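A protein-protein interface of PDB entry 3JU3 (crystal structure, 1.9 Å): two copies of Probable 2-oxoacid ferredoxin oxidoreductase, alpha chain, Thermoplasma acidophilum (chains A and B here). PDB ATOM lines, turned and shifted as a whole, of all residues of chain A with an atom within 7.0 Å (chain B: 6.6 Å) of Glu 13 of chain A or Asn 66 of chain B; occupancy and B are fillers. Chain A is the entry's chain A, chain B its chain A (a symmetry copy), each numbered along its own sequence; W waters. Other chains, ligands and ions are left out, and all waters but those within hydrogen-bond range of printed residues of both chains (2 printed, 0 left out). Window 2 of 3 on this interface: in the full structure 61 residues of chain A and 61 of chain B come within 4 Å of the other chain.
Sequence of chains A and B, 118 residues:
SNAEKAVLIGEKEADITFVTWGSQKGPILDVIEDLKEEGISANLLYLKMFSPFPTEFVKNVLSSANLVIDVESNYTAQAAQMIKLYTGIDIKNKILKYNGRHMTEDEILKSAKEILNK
Hydrophobic or aromatic side chains of chain B that line the printed part of chain A: Ala 65, Leu 67 and Val 68. Of the 12 printed residues of chain A, 5 touch a printed residue of chain B. Among the printed residues, 8 pairs touch across the chains. Among the printed residues, no Asp or Glu carboxylate lies within 4 Å of a Lys or Arg side-chain nitrogen of the other chain.
The side-chain carboxylate (OD2) of Asp 15 of chain A is in hydrogen-bond range of the backbone NH (N) of Ser 41 of chain A (3.0 Å). N of Ile 16 of chain A sits at hydrogen-bond distance from O of Ser 41 of chain A (3.2 Å). The backbone carbonyl oxygen (O) of Ile 16 of chain A lies within hydrogen-bond range of the backbone NH (N) of Asn 43 of chain A (2.9 Å). The side-chain hydroxyl (OG1) of Thr 17 of chain A lies within hydrogen-bond range of the side-chain amide oxygen (OD1) of Asn 43 of chain A, at 2.7 Å.
Of the printed residues of chain B, Glu 13 of chain A touches Asn 66 (3.7 Å). Printed residues of chain A within 4 Å of Asn 66 of chain B: Glu 13 (3.7 Å), Ala 14 (3.2 Å) and Asp 15 (3.8 Å). Of the printed residues of chain A, Val 68 of chain B touches Thr 17 (3.3 Å). Of the printed residues of chain B, Asp 15 of chain A touches Asn 66 and Leu 67. Of the printed residues of chain A, Leu 67 of chain B touches Asp 15 (3.6 Å), Ile 16 (3.6 Å) and Thr 17 (2.8 Å). Of the printed residues of chain A, Ala 65 of chain B touches Thr 17. Printed residues of chain B within 4 Å of Thr 17 of chain A: Ala 65, Leu 67 and Val 68.
The side-chain amide nitrogen of Asn 66 of chain B is in hydrogen-bond range of the backbone carbonyl oxygen of Ala 14 of chain A. O of Leu 67 of chain B sits at hydrogen-bond distance from N of Thr 17 of chain A (2.8 Å).
Asn 66 of chain B touches Glu 13 of chain A. O of Asp 15 of chain A touches CB of Asn 66 of chain B, 3.8 Å away. O of Asp 15 of chain A touches CB of Leu 67 of chain B, at 3.6 Å. Ile 16 of chain A touches Leu 67 of chain B. Thr 17 of chain A touches Ala 65 of chain B. CA of Val 68 of chain B touches O of Thr 17 of chain A, 3.3 Å away.
Water W1 lies within hydrogen-bond range of OE2 of Glu 13 of chain A (2.5 Å) and ND2 of Asn 66 of chain B (3.2 Å). Water W2 lies within hydrogen-bond range of O of Ala 14 of chain A (2.9 Å), OG1 of Thr 17 of chain A (3.0 Å), N of Asn 66 of chain B (3.0 Å) and N of Leu 67 of chain B (3.1 Å).
No position is printed for both chains.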
ATOM      1  N   LEU A   8     -24.487   5.662  17.650  1.00  0.00           N
ATOM      2  CA  LEU A   8     -23.782   6.529  18.581  1.00  0.00           C
ATOM      3  C   LEU A   8     -24.647   7.767  18.724  1.00  0.00           C
ATOM      4  O   LEU A   8     -24.815   8.488  17.751  1.00  0.00           O
ATOM      5  CB  LEU A   8     -22.411   6.933  18.025  1.00  0.00           C
ATOM      6  CG  LEU A   8     -21.590   7.826  18.955  1.00  0.00           C
ATOM      7  CD1 LEU A   8     -21.256   7.134  20.282  1.00  0.00           C
ATOM      8  CD2 LEU A   8     -20.331   8.310  18.263  1.00  0.00           C
ATOM      9  N   GLY A  10     -25.308  11.452  20.281  1.00  0.00           N
ATOM     10  CA  GLY A  10     -24.555  12.603  20.749  1.00  0.00           C
ATOM     11  C   GLY A  10     -23.404  12.942  19.819  1.00  0.00           C
ATOM     12  O   GLY A  10     -23.385  12.593  18.638  1.00  0.00           O
ATOM     13  N   GLU A  11     -22.428  13.611  20.389  1.00  0.00           N
ATOM     14  CA  GLU A  11     -21.275  14.089  19.681  1.00  0.00           C
ATOM     15  C   GLU A  11     -20.212  13.020  19.504  1.00  0.00           C
ATOM     16  O   GLU A  11     -19.979  12.243  20.422  1.00  0.00           O
ATOM     17  CB  GLU A  11     -20.708  15.245  20.483  1.00  0.00           C
ATOM     18  CG  GLU A  11     -21.674  16.404  20.628  1.00  0.00           C
ATOM     19  CD  GLU A  11     -22.124  16.992  19.293  1.00  0.00           C
ATOM     20  OE1 GLU A  11     -21.255  17.372  18.467  1.00  0.00           O
ATOM     21  OE2 GLU A  11     -23.361  17.078  19.078  1.00  0.00           O
ATOM     22  N   LYS A  12     -19.554  13.000  18.339  1.00  0.00           N
ATOM     23  CA  LYS A  12     -18.524  11.994  18.031  1.00  0.00           C
ATOM     24  C   LYS A  12     -17.426  11.924  19.080  1.00  0.00           C
ATOM     25  O   LYS A  12     -17.047  10.833  19.493  1.00  0.00           O
ATOM     26  CB  LYS A  12     -17.882  12.229  16.670  1.00  0.00           C
ATOM     27  CG  LYS A  12     -18.838  12.189  15.490  1.00  0.00           C
ATOM     28  CD  LYS A  12     -19.304  10.770  15.204  1.00  0.00           C
ATOM     29  CE  LYS A  12     -20.801  10.761  14.961  1.00  0.00           C
ATOM     30  NZ  LYS A  12     -21.279   9.396  14.644  1.00  0.00           N
ATOM     31  N   GLU A  13     -16.889  13.083  19.453  1.00  0.00           N
ATOM     32  CA  GLU A  13     -15.894  13.196  20.509  1.00  0.00           C
ATOM     33  C   GLU A  13     -16.680  13.560  21.741  1.00  0.00           C
ATOM     34  O   GLU A  13     -17.644  14.329  21.641  1.00  0.00           O
ATOM     35  CB  GLU A  13     -14.901  14.319  20.199  1.00  0.00           C
ATOM     36  CG  GLU A  13     -14.056  14.796  21.391  1.00  0.00           C
ATOM     37  CD  GLU A  13     -12.685  14.117  21.486  1.00  0.00           C
ATOM     38  OE1 GLU A  13     -12.517  12.991  20.960  1.00  0.00           O
ATOM     39  OE2 GLU A  13     -11.771  14.719  22.087  1.00  0.00           O
ATOM     40  N   ALA A  14     -16.302  12.991  22.881  1.00  0.00           N
ATOM     41  CA  ALA A  14     -16.895  13.403  24.154  1.00  0.00           C
ATOM     42  C   ALA A  14     -15.981  13.026  25.275  1.00  0.00           C
ATOM     43  O   ALA A  14     -15.175  12.130  25.123  1.00  0.00           O
ATOM     44  CB  ALA A  14     -18.250  12.754  24.345  1.00  0.00           C
ATOM     45  N   ASP A  15     -16.078  13.735  26.383  1.00  0.00           N
ATOM     46  CA  ASP A  15     -15.331  13.418  27.583  1.00  0.00           C
ATOM     47  C   ASP A  15     -15.572  11.972  28.071  1.00  0.00           C
ATOM     48  O   ASP A  15     -14.651  11.322  28.546  1.00  0.00           O
ATOM     49  CB  ASP A  15     -15.703  14.403  28.694  1.00  0.00           C
ATOM     50  CG  ASP A  15     -15.270  15.848  28.374  1.00  0.00           C
ATOM     51  OD1 ASP A  15     -14.177  16.057  27.821  1.00  0.00           O
ATOM     52  OD2 ASP A  15     -16.045  16.782  28.649  1.00  0.00           O
ATOM     53  N   ILE A  16     -16.831  11.525  27.990  1.00  0.00           N
ATOM     54  CA  ILE A  16     -17.294  10.204  28.447  1.00  0.00           C
ATOM     55  C   ILE A  16     -18.104   9.547  27.321  1.00  0.00           C
ATOM     56  O   ILE A  16     -18.993  10.190  26.729  1.00  0.00           O
ATOM     57  CB  ILE A  16     -18.234  10.316  29.682  1.00  0.00           C
ATOM     58  CG1 ILE A  16     -17.469  10.850  30.914  1.00  0.00           C
ATOM     59  CG2 ILE A  16     -18.903   8.919  29.988  1.00  0.00           C
ATOM     60  CD1 ILE A  16     -18.359  11.432  32.032  1.00  0.00           C
ATOM     61  N   THR A  17     -17.824   8.268  27.047  1.00  0.00           N
ATOM     62  CA  THR A  17     -18.663   7.485  26.159  1.00  0.00           C
ATOM     63  C   THR A  17     -19.337   6.374  26.961  1.00  0.00           C
ATOM     64  O   THR A  17     -18.693   5.391  27.370  1.00  0.00           O
ATOM     65  CB  THR A  17     -17.789   6.883  25.020  1.00  0.00           C
ATOM     66  OG1 THR A  17     -17.333   7.957  24.199  1.00  0.00           O
ATOM     67  CG2 THR A  17     -18.570   5.850  24.132  1.00  0.00           C
ATOM     68  N   SER A  41     -18.995  16.812  28.383  1.00  0.00           N
ATOM     69  CA  SER A  41     -19.666  16.204  27.227  1.00  0.00           C
ATOM     70  C   SER A  41     -19.686  14.679  27.325  1.00  0.00           C
ATOM     71  O   SER A  41     -18.771  14.057  27.840  1.00  0.00           O
ATOM     72  CB  SER A  41     -19.017  16.647  25.910  1.00  0.00           C
ATOM     73  OG  SER A  41     -17.660  16.244  25.911  1.00  0.00           O
ATOM     74  N   ALA A  42     -20.730  14.063  26.788  1.00  0.00           N
ATOM     75  CA  ALA A  42     -20.823  12.620  26.890  1.00  0.00           C
ATOM     76  C   ALA A  42     -21.613  12.174  25.687  1.00  0.00           C
ATOM     77  O   ALA A  42     -22.492  12.916  25.202  1.00  0.00           O
ATOM     78  CB  ALA A  42     -21.481  12.223  28.202  1.00  0.00           C
ATOM     79  N   ASN A  43     -21.283  10.998  25.167  1.00  0.00           N
ATOM     80  CA  ASN A  43     -22.112  10.422  24.130  1.00  0.00           C
ATOM     81  C   ASN A  43     -22.519   8.998  24.564  1.00  0.00           C
ATOM     82  O   ASN A  43     -22.123   8.548  25.654  1.00  0.00           O
ATOM     83  CB  ASN A  43     -21.428  10.501  22.740  1.00  0.00           C
ATOM     84  CG  ASN A  43     -20.052   9.825  22.711  1.00  0.00           C
ATOM     85  OD1 ASN A  43     -19.732   9.032  23.590  1.00  0.00           O
ATOM     86  ND2 ASN A  43     -19.239  10.143  21.706  1.00  0.00           N
ATOM     87  N   LEU B  62     -15.159   2.800  19.929  1.00  0.00           N
ATOM     88  CA  LEU B  62     -14.543   2.699  21.247  1.00  0.00           C
ATOM     89  C   LEU B  62     -13.036   2.918  21.161  1.00  0.00           C
ATOM     90  O   LEU B  62     -12.398   3.416  22.116  1.00  0.00           O
ATOM     91  CB  LEU B  62     -14.871   1.358  21.900  1.00  0.00           C
ATOM     92  CG  LEU B  62     -16.344   1.110  22.267  1.00  0.00           C
ATOM     93  CD1 LEU B  62     -16.456  -0.176  23.018  1.00  0.00           C
ATOM     94  CD2 LEU B  62     -16.965   2.248  23.082  1.00  0.00           C
ATOM     95  N   SER B  64     -11.348   5.119  19.602  1.00  0.00           N
ATOM     96  CA  SER B  64     -10.945   6.540  19.688  1.00  0.00           C
ATOM     97  C   SER B  64     -11.552   7.306  20.876  1.00  0.00           C
ATOM     98  O   SER B  64     -11.314   8.505  21.038  1.00  0.00           O
ATOM     99  CB  SER B  64     -11.224   7.282  18.362  1.00  0.00           C
ATOM    100  OG  SER B  64     -12.485   6.899  17.814  1.00  0.00           O
ATOM    101  N   ALA B  65     -12.303   6.607  21.722  1.00  0.00           N
ATOM    102  CA  ALA B  65     -12.922   7.253  22.884  1.00  0.00           C
ATOM    103  C   ALA B  65     -11.917   7.657  23.978  1.00  0.00           C
ATOM    104  O   ALA B  65     -10.981   6.918  24.267  1.00  0.00           O
ATOM    105  CB  ALA B  65     -14.031   6.406  23.472  1.00  0.00           C
ATOM    106  N   ASN B  66     -12.116   8.834  24.584  1.00  0.00           N
ATOM    107  CA  ASN B  66     -11.314   9.231  25.761  1.00  0.00           C
ATOM    108  C   ASN B  66     -11.504   8.295  26.927  1.00  0.00           C
ATOM    109  O   ASN B  66     -10.549   7.924  27.596  1.00  0.00           O
ATOM    110  CB  ASN B  66     -11.654  10.651  26.247  1.00  0.00           C
ATOM    111  CG  ASN B  66     -11.253  11.694  25.279  1.00  0.00           C
ATOM    112  OD1 ASN B  66     -10.232  11.569  24.597  1.00  0.00           O
ATOM    113  ND2 ASN B  66     -12.025  12.762  25.220  1.00  0.00           N
ATOM    114  N   LEU B  67     -12.757   7.957  27.198  1.00  0.00           N
ATOM    115  CA  LEU B  67     -13.115   7.231  28.421  1.00  0.00           C
ATOM    116  C   LEU B  67     -14.428   6.504  28.215  1.00  0.00           C
ATOM    117  O   LEU B  67     -15.421   7.134  27.864  1.00  0.00           O
ATOM    118  CB  LEU B  67     -13.260   8.215  29.575  1.00  0.00           C
ATOM    119  CG  LEU B  67     -14.003   7.808  30.844  1.00  0.00           C
ATOM    120  CD1 LEU B  67     -13.275   6.682  31.482  1.00  0.00           C
ATOM    121  CD2 LEU B  67     -14.039   9.012  31.793  1.00  0.00           C
ATOM    122  N   VAL B  68     -14.437   5.187  28.438  1.00  0.00           N
ATOM    123  CA  VAL B  68     -15.621   4.386  28.165  1.00  0.00           C
ATOM    124  C   VAL B  68     -16.166   3.867  29.495  1.00  0.00           C
ATOM    125  O   VAL B  68     -15.389   3.379  30.338  1.00  0.00           O
ATOM    126  CB  VAL B  68     -15.289   3.204  27.246  1.00  0.00           C
ATOM    127  CG1 VAL B  68     -16.555   2.374  26.910  1.00  0.00           C
ATOM    128  CG2 VAL B  68     -14.612   3.676  25.938  1.00  0.00           C
HETATM  129  O   HOH W   1     -11.520  15.761  24.316  1.00  0.00           O
HETATM  130  O   HOH W   2     -14.968   9.264  25.466  1.00  0.00           O
